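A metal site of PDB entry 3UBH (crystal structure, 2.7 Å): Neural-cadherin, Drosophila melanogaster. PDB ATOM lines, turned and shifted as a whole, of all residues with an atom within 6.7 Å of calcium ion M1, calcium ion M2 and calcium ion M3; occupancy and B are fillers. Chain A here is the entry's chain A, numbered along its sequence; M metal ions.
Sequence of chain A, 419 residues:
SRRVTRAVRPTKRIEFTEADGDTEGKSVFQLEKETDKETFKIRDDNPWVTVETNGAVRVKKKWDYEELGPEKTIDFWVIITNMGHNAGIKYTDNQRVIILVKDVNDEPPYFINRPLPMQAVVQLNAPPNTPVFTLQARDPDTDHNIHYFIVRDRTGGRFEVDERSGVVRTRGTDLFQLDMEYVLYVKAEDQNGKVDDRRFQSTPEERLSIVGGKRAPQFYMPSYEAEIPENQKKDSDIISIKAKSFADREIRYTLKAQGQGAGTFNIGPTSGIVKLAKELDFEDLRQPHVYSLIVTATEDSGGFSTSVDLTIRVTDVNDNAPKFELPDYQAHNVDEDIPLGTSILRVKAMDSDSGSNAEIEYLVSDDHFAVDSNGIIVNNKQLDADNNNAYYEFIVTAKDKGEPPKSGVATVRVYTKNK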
ATOM      1  N   GLU A  18      -1.655  15.693 -22.603  1.00  0.00           N
ATOM      2  CA  GLU A  18      -0.787  16.485 -21.758  1.00  0.00           C
ATOM      3  C   GLU A  18      -0.820  16.028 -20.313  1.00  0.00           C
ATOM      4  O   GLU A  18       0.211  15.682 -19.741  1.00  0.00           O
ATOM      5  CB  GLU A  18      -1.321  17.910 -21.812  1.00  0.00           C
ATOM      6  CG  GLU A  18      -0.310  18.993 -21.832  1.00  0.00           C
ATOM      7  CD  GLU A  18      -0.955  20.324 -22.100  1.00  0.00           C
ATOM      8  OE1 GLU A  18      -2.155  20.339 -22.442  1.00  0.00           O
ATOM      9  OE2 GLU A  18      -0.268  21.353 -21.959  1.00  0.00           O
ATOM     10  N   TRP A  63       4.789  17.334 -19.229  1.00  0.00           N
ATOM     11  CA  TRP A  63       4.353  17.449 -20.613  1.00  0.00           C
ATOM     12  C   TRP A  63       3.485  18.688 -20.825  1.00  0.00           C
ATOM     13  O   TRP A  63       2.682  19.070 -19.966  1.00  0.00           O
ATOM     14  CB  TRP A  63       3.603  16.195 -21.032  1.00  0.00           C
ATOM     15  CG  TRP A  63       4.471  14.976 -21.148  1.00  0.00           C
ATOM     16  CD1 TRP A  63       5.816  14.873 -20.861  1.00  0.00           C
ATOM     17  CD2 TRP A  63       4.062  13.671 -21.547  1.00  0.00           C
ATOM     18  NE1 TRP A  63       6.250  13.588 -21.079  1.00  0.00           N
ATOM     19  CE2 TRP A  63       5.193  12.838 -21.502  1.00  0.00           C
ATOM     20  CE3 TRP A  63       2.827  13.127 -21.956  1.00  0.00           C
ATOM     21  CZ2 TRP A  63       5.147  11.492 -21.845  1.00  0.00           C
ATOM     22  CZ3 TRP A  63       2.781  11.782 -22.300  1.00  0.00           C
ATOM     23  CH2 TRP A  63       3.934  10.974 -22.225  1.00  0.00           C
ATOM     24  N   ASP A  64       3.687  19.322 -21.966  1.00  0.00           N
ATOM     25  CA  ASP A  64       3.068  20.611 -22.204  1.00  0.00           C
ATOM     26  C   ASP A  64       2.760  20.789 -23.679  1.00  0.00           C
ATOM     27  O   ASP A  64       3.667  20.976 -24.489  1.00  0.00           O
ATOM     28  CB  ASP A  64       3.999  21.713 -21.720  1.00  0.00           C
ATOM     29  CG  ASP A  64       3.266  23.002 -21.441  1.00  0.00           C
ATOM     30  OD1 ASP A  64       2.158  23.217 -21.976  1.00  0.00           O
ATOM     31  OD2 ASP A  64       3.812  23.803 -20.659  1.00  0.00           O
ATOM     32  N   TYR A  65       1.480  20.724 -24.010  1.00  0.00           N
ATOM     33  CA  TYR A  65       0.998  20.953 -25.357  1.00  0.00           C
ATOM     34  C   TYR A  65       1.383  22.336 -25.827  1.00  0.00           C
ATOM     35  O   TYR A  65       1.784  22.514 -26.968  1.00  0.00           O
ATOM     36  CB  TYR A  65      -0.519  20.778 -25.409  1.00  0.00           C
ATOM     37  CG  TYR A  65      -1.132  20.827 -26.799  1.00  0.00           C
ATOM     38  CD1 TYR A  65      -1.221  19.677 -27.573  1.00  0.00           C
ATOM     39  CD2 TYR A  65      -1.637  22.015 -27.317  1.00  0.00           C
ATOM     40  CE1 TYR A  65      -1.790  19.698 -28.845  1.00  0.00           C
ATOM     41  CE2 TYR A  65      -2.207  22.063 -28.598  1.00  0.00           C
ATOM     42  CZ  TYR A  65      -2.279  20.888 -29.356  1.00  0.00           C
ATOM     43  OH  TYR A  65      -2.837  20.909 -30.609  1.00  0.00           O
ATOM     44  N   GLU A  66       1.279  23.318 -24.936  1.00  0.00           N
ATOM     45  CA  GLU A  66       1.581  24.721 -25.244  1.00  0.00           C
ATOM     46  C   GLU A  66       3.059  24.983 -25.588  1.00  0.00           C
ATOM     47  O   GLU A  66       3.396  26.041 -26.091  1.00  0.00           O
ATOM     48  CB  GLU A  66       1.154  25.621 -24.075  1.00  0.00           C
ATOM     49  CG  GLU A  66      -0.340  25.861 -23.946  1.00  0.00           C
ATOM     50  CD  GLU A  66      -1.151  24.603 -23.610  1.00  0.00           C
ATOM     51  OE1 GLU A  66      -0.869  23.915 -22.607  1.00  0.00           O
ATOM     52  OE2 GLU A  66      -2.098  24.312 -24.367  1.00  0.00           O
ATOM     53  N   GLU A  67       3.935  24.016 -25.316  1.00  0.00           N
ATOM     54  CA  GLU A  67       5.370  24.237 -25.508  1.00  0.00           C
ATOM     55  C   GLU A  67       5.983  23.310 -26.568  1.00  0.00           C
ATOM     56  O   GLU A  67       7.158  23.410 -26.881  1.00  0.00           O
ATOM     57  CB  GLU A  67       6.119  24.133 -24.183  1.00  0.00           C
ATOM     58  CG  GLU A  67       7.083  25.301 -23.911  1.00  0.00           C
ATOM     59  CD  GLU A  67       8.492  24.846 -23.522  1.00  0.00           C
ATOM     60  OE1 GLU A  67       8.637  23.798 -22.844  1.00  0.00           O
ATOM     61  OE2 GLU A  67       9.458  25.555 -23.915  1.00  0.00           O
ATOM     62  N   LYS A 102      -2.119  15.170 -26.842  1.00  0.00           N
ATOM     63  CA  LYS A 102      -3.380  15.901 -27.008  1.00  0.00           C
ATOM     64  C   LYS A 102      -3.544  17.061 -26.023  1.00  0.00           C
ATOM     65  O   LYS A 102      -3.115  16.984 -24.865  1.00  0.00           O
ATOM     66  CB  LYS A 102      -4.571  14.936 -26.978  1.00  0.00           C
ATOM     67  CG  LYS A 102      -4.674  14.060 -28.236  1.00  0.00           C
ATOM     68  CD  LYS A 102      -5.229  14.833 -29.435  1.00  0.00           C
ATOM     69  CE  LYS A 102      -4.528  14.425 -30.737  1.00  0.00           C
ATOM     70  NZ  LYS A 102      -5.315  14.802 -31.971  1.00  0.00           N
ATOM     71  N   ASP A 103      -4.154  18.132 -26.502  1.00  0.00           N
ATOM     72  CA  ASP A 103      -4.353  19.337 -25.696  1.00  0.00           C
ATOM     73  C   ASP A 103      -5.322  19.126 -24.543  1.00  0.00           C
ATOM     74  O   ASP A 103      -6.310  18.409 -24.658  1.00  0.00           O
ATOM     75  CB  ASP A 103      -4.837  20.505 -26.578  1.00  0.00           C
ATOM     76  CG  ASP A 103      -4.707  21.859 -25.890  1.00  0.00           C
ATOM     77  OD1 ASP A 103      -3.888  22.011 -24.953  1.00  0.00           O
ATOM     78  OD2 ASP A 103      -5.436  22.789 -26.288  1.00  0.00           O
ATOM     79  N   VAL A 104      -4.997  19.742 -23.418  1.00  0.00           N
ATOM     80  CA  VAL A 104      -5.910  19.856 -22.297  1.00  0.00           C
ATOM     81  C   VAL A 104      -5.923  21.330 -21.919  1.00  0.00           C
ATOM     82  O   VAL A 104      -4.876  21.983 -21.892  1.00  0.00           O
ATOM     83  CB  VAL A 104      -5.461  18.993 -21.068  1.00  0.00           C
ATOM     84  CG1 VAL A 104      -6.410  19.177 -19.888  1.00  0.00           C
ATOM     85  CG2 VAL A 104      -5.365  17.532 -21.436  1.00  0.00           C
ATOM     86  N   ASN A 105      -7.117  21.851 -21.634  1.00  0.00           N
ATOM     87  CA  ASN A 105      -7.256  23.200 -21.102  1.00  0.00           C
ATOM     88  C   ASN A 105      -6.656  23.298 -19.694  1.00  0.00           C
ATOM     89  O   ASN A 105      -7.372  23.170 -18.696  1.00  0.00           O
ATOM     90  CB  ASN A 105      -8.721  23.599 -21.106  1.00  0.00           C
ATOM     91  CG  ASN A 105      -8.916  25.071 -20.882  1.00  0.00           C
ATOM     92  OD1 ASN A 105      -8.185  25.701 -20.116  1.00  0.00           O
ATOM     93  ND2 ASN A 105      -9.921  25.648 -21.546  1.00  0.00           N
ATOM     94  N   ASP A 106      -5.353  23.558 -19.614  1.00  0.00           N
ATOM     95  CA  ASP A 106      -4.617  23.420 -18.350  1.00  0.00           C
ATOM     96  C   ASP A 106      -3.871  24.684 -17.923  1.00  0.00           C
ATOM     97  O   ASP A 106      -3.176  24.692 -16.892  1.00  0.00           O
ATOM     98  CB  ASP A 106      -3.629  22.253 -18.455  1.00  0.00           C
ATOM     99  CG  ASP A 106      -2.506  22.494 -19.457  1.00  0.00           C
ATOM    100  OD1 ASP A 106      -2.741  23.092 -20.537  1.00  0.00           O
ATOM    101  OD2 ASP A 106      -1.369  22.080 -19.175  1.00  0.00           O
ATOM    102  N   GLU A 107      -4.012  25.752 -18.726  1.00  0.00           N
ATOM    103  CA  GLU A 107      -3.346  27.019 -18.444  1.00  0.00           C
ATOM    104  C   GLU A 107      -4.375  28.113 -18.242  1.00  0.00           C
ATOM    105  O   GLU A 107      -5.313  28.243 -19.031  1.00  0.00           O
ATOM    106  CB  GLU A 107      -2.421  27.399 -19.601  1.00  0.00           C
ATOM    107  CG  GLU A 107      -1.521  26.282 -20.122  1.00  0.00           C
ATOM    108  CD  GLU A 107      -0.526  25.747 -19.116  1.00  0.00           C
ATOM    109  OE1 GLU A 107      -0.185  26.446 -18.150  1.00  0.00           O
ATOM    110  OE2 GLU A 107      -0.072  24.601 -19.297  1.00  0.00           O
ATOM    111  N   PRO A 108      -4.211  28.917 -17.166  1.00  0.00           N
ATOM    112  CA  PRO A 108      -5.178  29.974 -16.826  1.00  0.00           C
ATOM    113  C   PRO A 108      -5.083  31.166 -17.773  1.00  0.00           C
ATOM    114  O   PRO A 108      -4.026  31.371 -18.374  1.00  0.00           O
ATOM    115  CB  PRO A 108      -4.727  30.419 -15.436  1.00  0.00           C
ATOM    116  CG  PRO A 108      -3.239  30.132 -15.408  1.00  0.00           C
ATOM    117  CD  PRO A 108      -3.073  28.878 -16.224  1.00  0.00           C
ATOM    118  N   PRO A 109      -6.172  31.948 -17.885  1.00  0.00           N
ATOM    119  CA  PRO A 109      -6.176  33.157 -18.678  1.00  0.00           C
ATOM    120  C   PRO A 109      -5.412  34.273 -17.949  1.00  0.00           C
ATOM    121  O   PRO A 109      -5.143  34.139 -16.749  1.00  0.00           O
ATOM    122  CB  PRO A 109      -7.664  33.495 -18.754  1.00  0.00           C
ATOM    123  CG  PRO A 109      -8.217  33.001 -17.520  1.00  0.00           C
ATOM    124  CD  PRO A 109      -7.485  31.729 -17.258  1.00  0.00           C
ATOM    125  N   ASP A 139      -5.554  33.470 -23.386  1.00  0.00           N
ATOM    126  CA  ASP A 139      -5.482  32.136 -22.804  1.00  0.00           C
ATOM    127  C   ASP A 139      -4.729  31.207 -23.742  1.00  0.00           C
ATOM    128  O   ASP A 139      -5.111  31.058 -24.911  1.00  0.00           O
ATOM    129  CB  ASP A 139      -6.878  31.594 -22.504  1.00  0.00           C
ATOM    130  CG  ASP A 139      -6.853  30.259 -21.760  1.00  0.00           C
ATOM    131  OD1 ASP A 139      -6.455  29.237 -22.357  1.00  0.00           O
ATOM    132  OD2 ASP A 139      -7.224  30.232 -20.568  1.00  0.00           O
ATOM    133  N   PRO A 140      -3.673  30.564 -23.239  1.00  0.00           N
ATOM    134  CA  PRO A 140      -2.774  29.770 -24.048  1.00  0.00           C
ATOM    135  C   PRO A 140      -3.419  28.553 -24.705  1.00  0.00           C
ATOM    136  O   PRO A 140      -2.884  28.069 -25.700  1.00  0.00           O
ATOM    137  CB  PRO A 140      -1.697  29.319 -23.044  1.00  0.00           C
ATOM    138  CG  PRO A 140      -1.786  30.256 -21.926  1.00  0.00           C
ATOM    139  CD  PRO A 140      -3.248  30.583 -21.832  1.00  0.00           C
ATOM    140  N   ASP A 141      -4.525  28.050 -24.146  1.00  0.00           N
ATOM    141  CA  ASP A 141      -5.155  26.812 -24.617  1.00  0.00           C
ATOM    142  C   ASP A 141      -5.931  27.007 -25.912  1.00  0.00           C
ATOM    143  O   ASP A 141      -6.472  28.076 -26.148  1.00  0.00           O
ATOM    144  CB  ASP A 141      -6.083  26.234 -23.545  1.00  0.00           C
ATOM    145  CG  ASP A 141      -5.340  25.693 -22.355  1.00  0.00           C
ATOM    146  OD1 ASP A 141      -5.503  26.253 -21.248  1.00  0.00           O
ATOM    147  OD2 ASP A 141      -4.584  24.714 -22.504  1.00  0.00           O
ATOM    148  N   THR A 142      -5.995  25.963 -26.726  1.00  0.00           N
ATOM    149  CA  THR A 142      -6.590  26.037 -28.063  1.00  0.00           C
ATOM    150  C   THR A 142      -8.076  26.399 -28.062  1.00  0.00           C
ATOM    151  O   THR A 142      -8.521  27.262 -28.830  1.00  0.00           O
ATOM    152  CB  THR A 142      -6.376  24.720 -28.847  1.00  0.00           C
ATOM    153  OG1 THR A 142      -6.863  23.612 -28.070  1.00  0.00           O
ATOM    154  CG2 THR A 142      -4.889  24.507 -29.166  1.00  0.00           C
ATOM    155  N   ASP A 143      -8.840  25.752 -27.174  1.00  0.00           N
ATOM    156  CA  ASP A 143     -10.292  25.915 -27.103  1.00  0.00           C
ATOM    157  C   ASP A 143     -10.789  26.825 -25.966  1.00  0.00           C
ATOM    158  O   ASP A 143     -11.867  26.605 -25.431  1.00  0.00           O
ATOM    159  CB  ASP A 143     -10.957  24.535 -26.994  1.00  0.00           C
ATOM    160  CG  ASP A 143     -10.811  23.898 -25.593  1.00  0.00           C
ATOM    161  OD1 ASP A 143     -11.763  23.208 -25.167  1.00  0.00           O
ATOM    162  OD2 ASP A 143      -9.750  24.066 -24.927  1.00  0.00           O
ATOM    163  N   HIS A 144     -10.018  27.863 -25.621  1.00  0.00           N
ATOM    164  CA  HIS A 144     -10.397  28.787 -24.545  1.00  0.00           C
ATOM    165  C   HIS A 144     -11.769  29.462 -24.713  1.00  0.00           C
ATOM    166  O   HIS A 144     -12.316  29.539 -25.814  1.00  0.00           O
ATOM    167  CB  HIS A 144      -9.329  29.852 -24.346  1.00  0.00           C
ATOM    168  CG  HIS A 144      -9.123  30.727 -25.545  1.00  0.00           C
ATOM    169  ND1 HIS A 144     -10.028  31.694 -25.929  1.00  0.00           N
ATOM    170  CD2 HIS A 144      -8.098  30.797 -26.428  1.00  0.00           C
ATOM    171  CE1 HIS A 144      -9.570  32.309 -27.010  1.00  0.00           C
ATOM    172  NE2 HIS A 144      -8.406  31.783 -27.330  1.00  0.00           N
ATOM    173  N   ASN A 145     -12.319  29.942 -23.617  1.00  0.00           N
ATOM    174  CA  ASN A 145     -13.650  30.519 -23.633  1.00  0.00           C
ATOM    175  C   ASN A 145     -13.710  31.606 -22.581  1.00  0.00           C
ATOM    176  O   ASN A 145     -14.167  31.384 -21.457  1.00  0.00           O
ATOM    177  CB  ASN A 145     -14.710  29.440 -23.389  1.00  0.00           C
ATOM    178  CG  ASN A 145     -16.125  29.960 -23.529  1.00  0.00           C
ATOM    179  OD1 ASN A 145     -16.356  31.131 -23.864  1.00  0.00           O
ATOM    180  ND2 ASN A 145     -17.093  29.090 -23.265  1.00  0.00           N
ATOM    181  N   ASP A 190     -11.801  31.315 -17.919  1.00  0.00           N
ATOM    182  CA  ASP A 190     -11.883  30.442 -19.075  1.00  0.00           C
ATOM    183  C   ASP A 190     -12.825  29.312 -18.700  1.00  0.00           C
ATOM    184  O   ASP A 190     -12.497  28.466 -17.870  1.00  0.00           O
ATOM    185  CB  ASP A 190     -10.481  29.924 -19.437  1.00  0.00           C
ATOM    186  CG  ASP A 190     -10.504  28.915 -20.561  1.00  0.00           C
ATOM    187  OD1 ASP A 190     -11.538  28.759 -21.237  1.00  0.00           O
ATOM    188  OD2 ASP A 190      -9.444  28.281 -20.770  1.00  0.00           O
ATOM    189  N   ASN A 192     -13.980  26.866 -20.457  1.00  0.00           N
ATOM    190  CA  ASN A 192     -13.717  25.566 -21.030  1.00  0.00           C
ATOM    191  C   ASN A 192     -12.735  24.772 -20.183  1.00  0.00           C
ATOM    192  O   ASN A 192     -12.526  23.584 -20.429  1.00  0.00           O
ATOM    193  CB  ASN A 192     -13.257  25.698 -22.480  1.00  0.00           C
ATOM    194  CG  ASN A 192     -14.420  25.822 -23.456  1.00  0.00           C
ATOM    195  OD1 ASN A 192     -15.552  26.115 -23.077  1.00  0.00           O
ATOM    196  ND2 ASN A 192     -14.140  25.604 -24.731  1.00  0.00           N
ATOM    197  N   GLY A 193     -12.150  25.423 -19.178  1.00  0.00           N
ATOM    198  CA  GLY A 193     -11.256  24.754 -18.214  1.00  0.00           C
ATOM    199  C   GLY A 193     -11.581  25.006 -16.736  1.00  0.00           C
ATOM    200  O   GLY A 193     -11.970  26.112 -16.362  1.00  0.00           O
ATOM    201  N   GLN A 201     -10.994  28.101 -14.257  1.00  0.00           N
ATOM    202  CA  GLN A 201      -9.705  28.780 -14.397  1.00  0.00           C
ATOM    203  C   GLN A 201      -9.959  30.277 -14.437  1.00  0.00           C
ATOM    204  O   GLN A 201     -10.968  30.719 -14.991  1.00  0.00           O
ATOM    205  CB  GLN A 201      -9.026  28.407 -15.706  1.00  0.00           C
ATOM    206  CG  GLN A 201      -8.399  27.034 -15.774  1.00  0.00           C
ATOM    207  CD  GLN A 201      -7.880  26.759 -17.178  1.00  0.00           C
ATOM    208  OE1 GLN A 201      -7.910  27.646 -18.042  1.00  0.00           O
ATOM    209  NE2 GLN A 201      -7.424  25.550 -17.415  1.00  0.00           N
HETATM  210 CA    CA M   1      -7.242  27.932 -20.369  1.00  0.00          CA
HETATM  211 CA    CA M   2       0.318  22.890 -20.719  1.00  0.00          CA
HETATM  212 CA    CA M   3      -3.247  22.894 -22.909  1.00  0.00          CA
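Six residues have an atom within 4 Å of calcium ion M1: Asn 105, Glu 107, Asp 139, Asp 141, Asp 190 and Gln 201.
O of Val 104 is bound to calcium ion M3 (2.1 Å). OD2 of Asp 141 binds calcium ion M3 (2.3 Å). The side-chain carboxylate (OD1) of Asp 103 binds calcium ion M3 (2.3 Å). The side-chain carboxylate (OE2) of Glu 66 binds calcium ion M3 (2.3 Å). Calcium ion M3 is bound by OD1 of Asp 106 (2.4 Å). OE1 of Glu 66 binds calcium ion M3 (2.6 Å). OE1 of Glu 18 binds calcium ion M3, 2.8 Å away.
Six residues have an atom within 4 Å of calcium ion M3: Glu 18, Glu 66, Asp 103, Val 104, Asp 106 and Asp 141.
Calcium ion M2 is bound by OE2 of Glu 18, at 2.1 Å. Calcium ion M2 is bound by the side-chain carboxylate (OD1) of Asp 64, 2.3 Å away. OE2 of Glu 107 binds calcium ion M2, 2.3 Å away. Calcium ion M2 is bound by the side-chain carboxylate (OD2) of Asp 106. OE1 of Glu 66 binds calcium ion M2 (2.5 Å). Calcium ion M2 has five donor atoms within binding distance. Slightly farther from calcium ion M2 lies the side-chain carboxylate (OD1) of Asp 106 (3.1 Å).
The side-chain carboxylate (OE2) of Glu 18 sits close to the backbone NH (N) of Tyr 65 (2.8 Å). The backbone carbonyl oxygen of Lys 102 lies within hydrogen-bond range of the backbone NH of Glu 18 (3.0 Å). N of Asn 192 is in hydrogen-bond range of OD1 of Asp 190 (3.2 Å). The backbone NH of Asn 145 sits at hydrogen-bond distance from the side-chain carboxylate of Asp 190. The side-chain carboxylate of Asp 103 is in hydrogen-bond range of the side-chain hydroxyl of Thr 142 (2.4 Å). The side-chain amide nitrogen of Asn 105 sits close to the backbone NH of Gly 193 (3.3 Å). The backbone NH (N) of Gln 201 is in hydrogen-bond range of the backbone carbonyl oxygen (O) of Gly 193 (3.1 Å).
Five residues have an atom within 4 Å of calcium ion M2: Glu 18, Asp 64, Glu 66, Asp 106 and Glu 107. The nearest printed residue that does not touch calcium ion M2 is Tyr 65 (4.1 Å).
Calcium ion M1 is bound by the side-chain carboxylate (OD2) of Asp 190 (2.3 Å), the side-chain carboxylate (OD2) of Asp 139 (2.3 Å), the backbone carbonyl oxygen (O) of Glu 107 (2.4 Å), the side-chain amide oxygen (OD1) of Asn 105 (2.4 Å), the side-chain amide oxygen (OE1) of Gln 201 (2.4 Å), the side-chain carboxylate (OD1) of Asp 139 (2.5 Å) and the side-chain carboxylate (OD1) of Asp 141 (2.6 Å).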
